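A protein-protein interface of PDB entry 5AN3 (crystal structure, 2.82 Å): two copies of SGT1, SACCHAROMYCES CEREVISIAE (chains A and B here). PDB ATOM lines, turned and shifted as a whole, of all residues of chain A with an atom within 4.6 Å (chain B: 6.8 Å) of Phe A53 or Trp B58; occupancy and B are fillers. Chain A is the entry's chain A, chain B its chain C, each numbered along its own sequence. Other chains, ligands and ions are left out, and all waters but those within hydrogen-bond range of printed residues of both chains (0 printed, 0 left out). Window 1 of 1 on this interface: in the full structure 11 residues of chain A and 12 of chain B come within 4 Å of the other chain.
Tyr A52 touches Asp B57 (CE2 to O, 3.7 Å). Tyr A52 touches Trp B58 (O to CH2, 3.8 Å). Leu B48 touches Phe A53 (CD2 to O, 3.7 Å). Phe A53 touches Asp B57 (CE1 to O, 3.3 Å). CZ3 of Trp B58 touches O of Phe A53, 3.3 Å away. Ser B60 touches Phe A53 (CB to CE1, 3.5 Å). CB of Ala B62 touches CD2 of Phe A53, 3.4 Å away. Phe A53 touches Thr B63.
Of the printed residues of chain B, Lys A50 touches Asn B66 (3.0 Å). Of the printed residues of chain B, Asn A100 touches Ser B60 (2.9 Å). Phe B53 touches none of the printed residues of chain A. Of chain A, only Tyr A52 (3.8 Å), Phe A53 (3.3 Å) and His A59 (3.1 Å) come within 4 Å of Trp B58. His B59 touches none of the printed residues of chain A. The nearest residue of chain B that does not touch Phe A53 is His B59 (5.4 Å). The nearest printed residue of chain B that does not touch His A59 is Leu B21 (5.2 Å).
The side-chain amide nitrogen (ND2) of Asn B66 sits at hydrogen-bond distance from the backbone carbonyl oxygen (O) of Phe A53, at 3.0 Å. ND2 of Asn B66 lies within hydrogen-bond range of O of Lys A50 (3.0 Å). The backbone carbonyl oxygen (O) of Asn A100 sits at hydrogen-bond distance from the side-chain hydroxyl (OG) of Ser B60 (2.9 Å). A ring nitrogen (NE2) of His A59 lies within hydrogen-bond range of the indole nitrogen (NE1) of Trp B58, at 3.1 Å. A ring nitrogen (NE2) of His A59 lies within hydrogen-bond range of the side-chain carboxylate (OD2) of Asp B57 (2.8 Å). The backbone NH (N) of Gly A54 sits close to the side-chain amide nitrogen (ND2) of Asn B66 (3.4 Å).
Positions printed for both chains: 50, 51, 52, 53, 54, 55, 59 and 64. Of the 14 pairs that touch across the chains among the printed residues, none has its exchanged pair printed and touching as well.
O of Trp B58 sits at hydrogen-bond distance from OG1 of Thr B63. ND1 of His A59 lies within hydrogen-bond range of O of Tyr A52, 2.8 Å away. O of Ala B62 sits at hydrogen-bond distance from ND2 of Asn B66 (3.1 Å). The side-chain hydroxyl of Ser B60 lies close to the backbone NH of Ala B62 (3.3 Å).
Of the 21 printed residues of chain B, 7 touch a printed residue of chain A. Printed residues of chain B that touch a printed residue of chain A: Leu B48, Asp B57, Trp B58, Ser B60, Ala B62, Thr B63 and Asn B66. Printed residues of chain A that touch a printed residue of chain B: Lys A50, Tyr A52, Phe A53, Gly A54, His A59 and Asn A100. Hydrophobic or aromatic side chains of chain A that line the printed part of chain B: Tyr A52, Phe A53 and His A59. Among the printed residues, 14 pairs touch across the chains. Among the printed residues, no Asp or Glu carboxylate lies within 4 Å of a Lys or Arg side-chain nitrogen of the other chain.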
ATOM      1  N   GLU A  49     -10.453   4.645  20.373  1.00  0.00           N
ATOM      2  CA  GLU A  49      -9.179   5.251  19.994  1.00  0.00           C
ATOM      3  C   GLU A  49      -8.717   4.718  18.625  1.00  0.00           C
ATOM      4  O   GLU A  49      -8.230   5.499  17.815  1.00  0.00           O
ATOM      5  CB  GLU A  49      -8.099   5.010  21.050  1.00  0.00           C
ATOM      6  CG  GLU A  49      -8.319   5.740  22.367  1.00  0.00           C
ATOM      7  CD  GLU A  49      -7.288   5.436  23.446  1.00  0.00           C
ATOM      8  OE1 GLU A  49      -6.108   5.201  23.094  1.00  0.00           O
ATOM      9  OE2 GLU A  49      -7.658   5.451  24.643  1.00  0.00           O
ATOM     10  N   LYS A  50      -8.895   3.403  18.355  1.00  0.00           N
ATOM     11  CA  LYS A  50      -8.550   2.781  17.066  1.00  0.00           C
ATOM     12  C   LYS A  50      -9.443   3.333  15.934  1.00  0.00           C
ATOM     13  O   LYS A  50      -8.948   3.606  14.841  1.00  0.00           O
ATOM     14  CB  LYS A  50      -8.684   1.245  17.143  1.00  0.00           C
ATOM     15  CG  LYS A  50      -7.375   0.501  17.074  1.00  0.00           C
ATOM     16  CD  LYS A  50      -7.509  -0.740  16.208  1.00  0.00           C
ATOM     17  CE  LYS A  50      -6.146  -1.217  15.799  1.00  0.00           C
ATOM     18  N   LEU A  51     -10.760   3.483  16.207  1.00  0.00           N
ATOM     19  CA  LEU A  51     -11.750   3.982  15.244  1.00  0.00           C
ATOM     20  C   LEU A  51     -11.477   5.448  14.898  1.00  0.00           C
ATOM     21  O   LEU A  51     -11.539   5.813  13.727  1.00  0.00           O
ATOM     22  CB  LEU A  51     -13.178   3.813  15.777  1.00  0.00           C
ATOM     23  CG  LEU A  51     -13.676   2.372  16.005  1.00  0.00           C
ATOM     24  CD1 LEU A  51     -14.894   2.375  16.904  1.00  0.00           C
ATOM     25  CD2 LEU A  51     -13.986   1.672  14.698  1.00  0.00           C
ATOM     26  N   TYR A  52     -11.127   6.273  15.908  1.00  0.00           N
ATOM     27  CA  TYR A  52     -10.815   7.696  15.741  1.00  0.00           C
ATOM     28  C   TYR A  52      -9.751   7.861  14.677  1.00  0.00           C
ATOM     29  O   TYR A  52      -9.905   8.677  13.778  1.00  0.00           O
ATOM     30  CB  TYR A  52     -10.343   8.303  17.073  1.00  0.00           C
ATOM     31  CG  TYR A  52      -9.933   9.764  16.993  1.00  0.00           C
ATOM     32  CD1 TYR A  52     -10.871  10.778  17.107  1.00  0.00           C
ATOM     33  CD2 TYR A  52      -8.605  10.129  16.791  1.00  0.00           C
ATOM     34  CE1 TYR A  52     -10.505  12.113  17.002  1.00  0.00           C
ATOM     35  CE2 TYR A  52      -8.227  11.466  16.682  1.00  0.00           C
ATOM     36  CZ  TYR A  52      -9.182  12.456  16.789  1.00  0.00           C
ATOM     37  OH  TYR A  52      -8.833  13.784  16.684  1.00  0.00           O
ATOM     38  N   PHE A  53      -8.703   7.041  14.765  1.00  0.00           N
ATOM     39  CA  PHE A  53      -7.544   7.040  13.884  1.00  0.00           C
ATOM     40  C   PHE A  53      -7.660   6.106  12.676  1.00  0.00           C
ATOM     41  O   PHE A  53      -6.691   5.954  11.941  1.00  0.00           O
ATOM     42  CB  PHE A  53      -6.311   6.637  14.690  1.00  0.00           C
ATOM     43  CG  PHE A  53      -5.891   7.669  15.695  1.00  0.00           C
ATOM     44  CD1 PHE A  53      -5.441   8.932  15.284  1.00  0.00           C
ATOM     45  CD2 PHE A  53      -5.933   7.390  17.053  1.00  0.00           C
ATOM     46  CE1 PHE A  53      -5.045   9.890  16.220  1.00  0.00           C
ATOM     47  CE2 PHE A  53      -5.507   8.335  17.984  1.00  0.00           C
ATOM     48  CZ  PHE A  53      -5.060   9.579  17.564  1.00  0.00           C
ATOM     49  N   GLY A  54      -8.811   5.501  12.453  1.00  0.00           N
ATOM     50  CA  GLY A  54      -8.968   4.617  11.306  1.00  0.00           C
ATOM     51  C   GLY A  54     -10.182   4.852  10.430  1.00  0.00           C
ATOM     52  O   GLY A  54     -10.284   4.256   9.359  1.00  0.00           O
ATOM     53  N   PHE A  55     -11.119   5.686  10.881  1.00  0.00           N
ATOM     54  CA  PHE A  55     -12.365   5.929  10.168  1.00  0.00           C
ATOM     55  C   PHE A  55     -12.705   7.399  10.171  1.00  0.00           C
ATOM     56  O   PHE A  55     -12.624   8.054  11.214  1.00  0.00           O
ATOM     57  CB  PHE A  55     -13.501   5.119  10.820  1.00  0.00           C
ATOM     58  CG  PHE A  55     -13.376   3.619  10.692  1.00  0.00           C
ATOM     59  CD1 PHE A  55     -12.657   2.876  11.631  1.00  0.00           C
ATOM     60  CD2 PHE A  55     -13.983   2.946   9.646  1.00  0.00           C
ATOM     61  CE1 PHE A  55     -12.545   1.487  11.514  1.00  0.00           C
ATOM     62  CE2 PHE A  55     -13.851   1.559   9.518  1.00  0.00           C
ATOM     63  CZ  PHE A  55     -13.151   0.837  10.464  1.00  0.00           C
ATOM     64  N   HIS A  59     -13.593  10.039  13.328  1.00  0.00           N
ATOM     65  CA  HIS A  59     -12.550  11.008  13.590  1.00  0.00           C
ATOM     66  C   HIS A  59     -13.170  12.357  14.016  1.00  0.00           C
ATOM     67  O   HIS A  59     -13.334  13.271  13.187  1.00  0.00           O
ATOM     68  CB  HIS A  59     -11.639  11.151  12.368  1.00  0.00           C
ATOM     69  CG  HIS A  59     -10.411  11.938  12.657  1.00  0.00           C
ATOM     70  ND1 HIS A  59      -9.354  11.382  13.333  1.00  0.00           N
ATOM     71  CD2 HIS A  59     -10.107  13.213  12.336  1.00  0.00           C
ATOM     72  CE1 HIS A  59      -8.447  12.341  13.427  1.00  0.00           C
ATOM     73  NE2 HIS A  59      -8.853  13.459  12.834  1.00  0.00           N
ATOM     74  N   MET A  64     -12.753  10.821  21.091  1.00  0.00           N
ATOM     75  CA  MET A  64     -11.629  10.859  22.026  1.00  0.00           C
ATOM     76  C   MET A  64     -12.074  11.192  23.437  1.00  0.00           C
ATOM     77  O   MET A  64     -11.570  10.577  24.389  1.00  0.00           O
ATOM     78  CB  MET A  64     -10.507  11.789  21.559  1.00  0.00           C
ATOM     79  CG  MET A  64      -9.458  11.054  20.684  1.00  0.00           C
ATOM     80  SD  MET A  64      -8.846   9.458  21.355  1.00  0.00           S
ATOM     81  CE  MET A  64      -8.189   8.853  20.067  1.00  0.00           C
ATOM     82  N   ASN A 100      -0.834   8.282  22.069  1.00  0.00           N
ATOM     83  CA  ASN A 100      -1.502   8.375  20.776  1.00  0.00           C
ATOM     84  C   ASN A 100      -2.011   9.801  20.472  1.00  0.00           C
ATOM     85  O   ASN A 100      -2.022  10.187  19.308  1.00  0.00           O
ATOM     86  CB  ASN A 100      -2.645   7.392  20.716  1.00  0.00           C
ATOM     87  CG  ASN A 100      -2.207   5.960  20.683  1.00  0.00           C
ATOM     88  OD1 ASN A 100      -1.151   5.618  20.131  1.00  0.00           O
ATOM     89  ND2 ASN A 100      -3.078   5.083  21.176  1.00  0.00           N
ATOM     90  N   LEU B  21      -8.709  12.954   3.077  1.00  0.00           N
ATOM     91  CA  LEU B  21      -9.852  12.826   3.989  1.00  0.00           C
ATOM     92  C   LEU B  21     -11.157  12.480   3.220  1.00  0.00           C
ATOM     93  O   LEU B  21     -11.981  11.719   3.734  1.00  0.00           O
ATOM     94  CB  LEU B  21     -10.041  14.079   4.845  1.00  0.00           C
ATOM     95  CG  LEU B  21     -10.663  13.822   6.219  1.00  0.00           C
ATOM     96  CD1 LEU B  21      -9.750  12.996   7.118  1.00  0.00           C
ATOM     97  CD2 LEU B  21     -10.998  15.120   6.901  1.00  0.00           C
ATOM     98  N   LEU B  24     -10.658   8.870   2.017  1.00  0.00           N
ATOM     99  CA  LEU B  24     -10.815   7.952   3.154  1.00  0.00           C
ATOM    100  C   LEU B  24     -12.269   7.579   3.324  1.00  0.00           C
ATOM    101  O   LEU B  24     -12.579   6.379   3.352  1.00  0.00           O
ATOM    102  CB  LEU B  24     -10.269   8.543   4.470  1.00  0.00           C
ATOM    103  CG  LEU B  24     -10.365   7.634   5.706  1.00  0.00           C
ATOM    104  CD1 LEU B  24      -9.425   6.453   5.584  1.00  0.00           C
ATOM    105  CD2 LEU B  24     -10.076   8.397   6.976  1.00  0.00           C
ATOM    106  N   CYS B  47      -4.482   6.320   2.264  1.00  0.00           N
ATOM    107  CA  CYS B  47      -5.145   7.509   2.809  1.00  0.00           C
ATOM    108  C   CYS B  47      -4.637   7.782   4.180  1.00  0.00           C
ATOM    109  O   CYS B  47      -4.198   8.900   4.447  1.00  0.00           O
ATOM    110  CB  CYS B  47      -6.657   7.345   2.824  1.00  0.00           C
ATOM    111  SG  CYS B  47      -7.400   7.344   1.185  1.00  0.00           S
ATOM    112  N   LEU B  48      -4.682   6.760   5.048  1.00  0.00           N
ATOM    113  CA  LEU B  48      -4.237   6.854   6.438  1.00  0.00           C
ATOM    114  C   LEU B  48      -2.755   7.239   6.523  1.00  0.00           C
ATOM    115  O   LEU B  48      -2.383   8.047   7.376  1.00  0.00           O
ATOM    116  CB  LEU B  48      -4.497   5.543   7.198  1.00  0.00           C
ATOM    117  CG  LEU B  48      -5.932   5.117   7.400  1.00  0.00           C
ATOM    118  CD1 LEU B  48      -5.969   3.771   8.042  1.00  0.00           C
ATOM    119  CD2 LEU B  48      -6.689   6.113   8.277  1.00  0.00           C
ATOM    120  N   LYS B  50      -1.115   9.052   4.133  1.00  0.00           N
ATOM    121  CA  LYS B  50      -1.093  10.466   3.718  1.00  0.00           C
ATOM    122  C   LYS B  50      -1.538  11.412   4.846  1.00  0.00           C
ATOM    123  O   LYS B  50      -0.938  12.484   5.028  1.00  0.00           O
ATOM    124  CB  LYS B  50      -1.969  10.724   2.492  1.00  0.00           C
ATOM    125  CG  LYS B  50      -1.469  10.206   1.162  1.00  0.00           C
ATOM    126  CD  LYS B  50      -0.150  10.796   0.714  1.00  0.00           C
ATOM    127  CE  LYS B  50       0.394  10.120  -0.518  1.00  0.00           C
ATOM    128  NZ  LYS B  50       1.867   9.928  -0.385  1.00  0.00           N
ATOM    129  N   LEU B  51      -2.585  11.002   5.599  1.00  0.00           N
ATOM    130  CA  LEU B  51      -3.143  11.772   6.706  1.00  0.00           C
ATOM    131  C   LEU B  51      -2.138  11.859   7.841  1.00  0.00           C
ATOM    132  O   LEU B  51      -1.965  12.935   8.410  1.00  0.00           O
ATOM    133  CB  LEU B  51      -4.475  11.160   7.195  1.00  0.00           C
ATOM    134  CG  LEU B  51      -5.657  11.179   6.212  1.00  0.00           C
ATOM    135  CD1 LEU B  51      -6.751  10.214   6.638  1.00  0.00           C
ATOM    136  CD2 LEU B  51      -6.234  12.540   6.066  1.00  0.00           C
ATOM    137  N   TYR B  52      -1.450  10.736   8.147  1.00  0.00           N
ATOM    138  CA  TYR B  52      -0.421  10.655   9.191  1.00  0.00           C
ATOM    139  C   TYR B  52       0.611  11.757   8.982  1.00  0.00           C
ATOM    140  O   TYR B  52       0.927  12.494   9.920  1.00  0.00           O
ATOM    141  CB  TYR B  52       0.261   9.275   9.181  1.00  0.00           C
ATOM    142  CG  TYR B  52       1.383   9.138  10.186  1.00  0.00           C
ATOM    143  CD1 TYR B  52       1.123   8.774  11.501  1.00  0.00           C
ATOM    144  CD2 TYR B  52       2.709   9.377   9.826  1.00  0.00           C
ATOM    145  CE1 TYR B  52       2.145   8.654  12.436  1.00  0.00           C
ATOM    146  CE2 TYR B  52       3.744   9.273  10.759  1.00  0.00           C
ATOM    147  CZ  TYR B  52       3.453   8.910  12.062  1.00  0.00           C
ATOM    148  OH  TYR B  52       4.450   8.795  12.996  1.00  0.00           O
ATOM    149  N   PHE B  53       1.074  11.893   7.728  1.00  0.00           N
ATOM    150  CA  PHE B  53       2.092  12.840   7.312  1.00  0.00           C
ATOM    151  C   PHE B  53       1.569  14.212   6.900  1.00  0.00           C
ATOM    152  O   PHE B  53       2.375  15.047   6.508  1.00  0.00           O
ATOM    153  CB  PHE B  53       2.869  12.223   6.138  1.00  0.00           C
ATOM    154  CG  PHE B  53       3.731  11.058   6.539  1.00  0.00           C
ATOM    155  CD1 PHE B  53       4.792  11.233   7.420  1.00  0.00           C
ATOM    156  CD2 PHE B  53       3.503   9.794   6.014  1.00  0.00           C
ATOM    157  CE1 PHE B  53       5.582  10.161   7.798  1.00  0.00           C
ATOM    158  CE2 PHE B  53       4.303   8.721   6.371  1.00  0.00           C
ATOM    159  CZ  PHE B  53       5.329   8.908   7.275  1.00  0.00           C
ATOM    160  N   GLY B  54       0.274  14.458   6.987  1.00  0.00           N
ATOM    161  CA  GLY B  54      -0.267  15.747   6.581  1.00  0.00           C
ATOM    162  C   GLY B  54      -1.166  16.459   7.565  1.00  0.00           C
ATOM    163  O   GLY B  54      -1.515  17.619   7.340  1.00  0.00           O
ATOM    164  N   PHE B  55      -1.577  15.772   8.636  1.00  0.00           N
ATOM    165  CA  PHE B  55      -2.505  16.318   9.617  1.00  0.00           C
ATOM    166  C   PHE B  55      -2.038  16.020  11.024  1.00  0.00           C
ATOM    167  O   PHE B  55      -1.640  14.897  11.325  1.00  0.00           O
ATOM    168  CB  PHE B  55      -3.903  15.732   9.382  1.00  0.00           C
ATOM    169  CG  PHE B  55      -4.558  16.149   8.087  1.00  0.00           C
ATOM    170  CD1 PHE B  55      -4.315  15.452   6.906  1.00  0.00           C
ATOM    171  CD2 PHE B  55      -5.452  17.202   8.055  1.00  0.00           C
ATOM    172  CE1 PHE B  55      -4.915  15.842   5.711  1.00  0.00           C
ATOM    173  CE2 PHE B  55      -6.097  17.552   6.867  1.00  0.00           C
ATOM    174  CZ  PHE B  55      -5.823  16.870   5.705  1.00  0.00           C
ATOM    175  N   SER B  56      -2.065  17.034  11.882  1.00  0.00           N
ATOM    176  CA  SER B  56      -1.639  16.901  13.270  1.00  0.00           C
ATOM    177  C   SER B  56      -2.491  15.841  13.996  1.00  0.00           C
ATOM    178  O   SER B  56      -1.929  14.982  14.672  1.00  0.00           O
ATOM    179  CB  SER B  56      -1.739  18.253  13.977  1.00  0.00           C
ATOM    180  OG  SER B  56      -1.599  18.125  15.382  1.00  0.00           O
ATOM    181  N   ASP B  57      -3.838  15.899  13.807  1.00  0.00           N
ATOM    182  CA  ASP B  57      -4.863  15.060  14.430  1.00  0.00           C
ATOM    183  C   ASP B  57      -4.784  13.604  13.962  1.00  0.00           C
ATOM    184  O   ASP B  57      -5.407  12.732  14.568  1.00  0.00           O
ATOM    185  CB  ASP B  57      -6.275  15.653  14.186  1.00  0.00           C
ATOM    186  CG  ASP B  57      -6.542  16.266  12.807  1.00  0.00           C
ATOM    187  OD1 ASP B  57      -5.787  17.177  12.400  1.00  0.00           O
ATOM    188  OD2 ASP B  57      -7.552  15.888  12.176  1.00  0.00           O
ATOM    189  N   TRP B  58      -4.020  13.339  12.906  1.00  0.00           N
ATOM    190  CA  TRP B  58      -3.815  12.008  12.353  1.00  0.00           C
ATOM    191  C   TRP B  58      -2.395  11.510  12.578  1.00  0.00           C
ATOM    192  O   TRP B  58      -2.098  10.350  12.330  1.00  0.00           O
ATOM    193  CB  TRP B  58      -4.126  12.028  10.855  1.00  0.00           C
ATOM    194  CG  TRP B  58      -5.594  12.120  10.543  1.00  0.00           C
ATOM    195  CD1 TRP B  58      -6.303  13.249  10.257  1.00  0.00           C
ATOM    196  CD2 TRP B  58      -6.531  11.035  10.490  1.00  0.00           C
ATOM    197  NE1 TRP B  58      -7.620  12.932  10.006  1.00  0.00           N
ATOM    198  CE2 TRP B  58      -7.791  11.578  10.157  1.00  0.00           C
ATOM    199  CE3 TRP B  58      -6.435   9.652  10.704  1.00  0.00           C
ATOM    200  CZ2 TRP B  58      -8.943  10.781  10.005  1.00  0.00           C
ATOM    201  CZ3 TRP B  58      -7.582   8.869  10.584  1.00  0.00           C
ATOM    202  CH2 TRP B  58      -8.814   9.433  10.233  1.00  0.00           C
ATOM    203  N   HIS B  59      -1.507  12.383  13.034  1.00  0.00           N
ATOM    204  CA  HIS B  59      -0.105  12.048  13.255  1.00  0.00           C
ATOM    205  C   HIS B  59       0.043  11.319  14.584  1.00  0.00           C
ATOM    206  O   HIS B  59       0.372  11.909  15.611  1.00  0.00           O
ATOM    207  CB  HIS B  59       0.767  13.296  13.169  1.00  0.00           C
ATOM    208  CG  HIS B  59       2.224  12.983  13.111  1.00  0.00           C
ATOM    209  ND1 HIS B  59       2.820  12.490  11.955  1.00  0.00           N
ATOM    210  CD2 HIS B  59       3.157  13.070  14.080  1.00  0.00           C
ATOM    211  CE1 HIS B  59       4.088  12.308  12.262  1.00  0.00           C
ATOM    212  NE2 HIS B  59       4.336  12.640  13.528  1.00  0.00           N
ATOM    213  N   SER B  60      -0.245  10.010  14.529  1.00  0.00           N
ATOM    214  CA  SER B  60      -0.244   9.062  15.637  1.00  0.00           C
ATOM    215  C   SER B  60       0.157   7.666  15.166  1.00  0.00           C
ATOM    216  O   SER B  60      -0.185   7.267  14.049  1.00  0.00           O
ATOM    217  CB  SER B  60      -1.641   8.996  16.242  1.00  0.00           C
ATOM    218  OG  SER B  60      -1.754   8.054  17.292  1.00  0.00           O
ATOM    219  N   ASP B  61       0.797   6.893  16.064  1.00  0.00           N
ATOM    220  CA  ASP B  61       1.157   5.502  15.832  1.00  0.00           C
ATOM    221  C   ASP B  61      -0.089   4.677  15.490  1.00  0.00           C
ATOM    222  O   ASP B  61       0.003   3.757  14.676  1.00  0.00           O
ATOM    223  CB  ASP B  61       1.850   4.923  17.074  1.00  0.00           C
ATOM    224  CG  ASP B  61       3.225   5.503  17.363  1.00  0.00           C
ATOM    225  OD1 ASP B  61       3.897   5.951  16.403  1.00  0.00           O
ATOM    226  OD2 ASP B  61       3.645   5.481  18.548  1.00  0.00           O
ATOM    227  N   ALA B  62      -1.258   5.034  16.085  1.00  0.00           N
ATOM    228  CA  ALA B  62      -2.537   4.362  15.861  1.00  0.00           C
ATOM    229  C   ALA B  62      -2.940   4.439  14.389  1.00  0.00           C
ATOM    230  O   ALA B  62      -3.375   3.431  13.838  1.00  0.00           O
ATOM    231  CB  ALA B  62      -3.610   4.956  16.754  1.00  0.00           C
ATOM    232  N   THR B  63      -2.670   5.574  13.727  1.00  0.00           N
ATOM    233  CA  THR B  63      -2.956   5.743  12.295  1.00  0.00           C
ATOM    234  C   THR B  63      -2.050   4.819  11.435  1.00  0.00           C
ATOM    235  O   THR B  63      -2.523   4.228  10.460  1.00  0.00           O
ATOM    236  CB  THR B  63      -2.814   7.216  11.879  1.00  0.00           C
ATOM    237  OG1 THR B  63      -3.581   8.015  12.768  1.00  0.00           O
ATOM    238  CG2 THR B  63      -3.323   7.477  10.476  1.00  0.00           C
ATOM    239  N   MET B  64      -0.759   4.704  11.787  1.00  0.00           N
ATOM    240  CA  MET B  64       0.145   3.855  11.027  1.00  0.00           C
ATOM    241  C   MET B  64      -0.173   2.383  11.271  1.00  0.00           C
ATOM    242  O   MET B  64      -0.091   1.585  10.327  1.00  0.00           O
ATOM    243  CB  MET B  64       1.613   4.171  11.335  1.00  0.00           C
ATOM    244  CG  MET B  64       2.233   5.119  10.319  1.00  0.00           C
ATOM    245  SD  MET B  64       2.122   4.590   8.593  1.00  0.00           S
ATOM    246  CE  MET B  64       2.428   6.086   7.805  1.00  0.00           C
ATOM    247  N   ASN B  66      -3.209   1.125  12.057  1.00  0.00           N
ATOM    248  CA  ASN B  66      -4.420   0.894  11.272  1.00  0.00           C
ATOM    249  C   ASN B  66      -4.071   0.690   9.783  1.00  0.00           C
ATOM    250  O   ASN B  66      -4.577  -0.259   9.179  1.00  0.00           O
ATOM    251  CB  ASN B  66      -5.389   2.057  11.448  1.00  0.00           C
ATOM    252  CG  ASN B  66      -6.064   2.065  12.787  1.00  0.00           C
ATOM    253  OD1 ASN B  66      -6.311   1.036  13.391  1.00  0.00           O
ATOM    254  ND2 ASN B  66      -6.403   3.234  13.274  1.00  0.00           N
ATOM    255  N   ALA B  67      -3.173   1.529   9.210  1.00  0.00           N
ATOM    256  CA  ALA B  67      -2.701   1.372   7.823  1.00  0.00           C
ATOM    257  C   ALA B  67      -2.029  -0.014   7.617  1.00  0.00           C
ATOM    258  O   ALA B  67      -2.442  -0.762   6.728  1.00  0.00           O
ATOM    259  CB  ALA B  67      -1.739   2.480   7.464  1.00  0.00           C
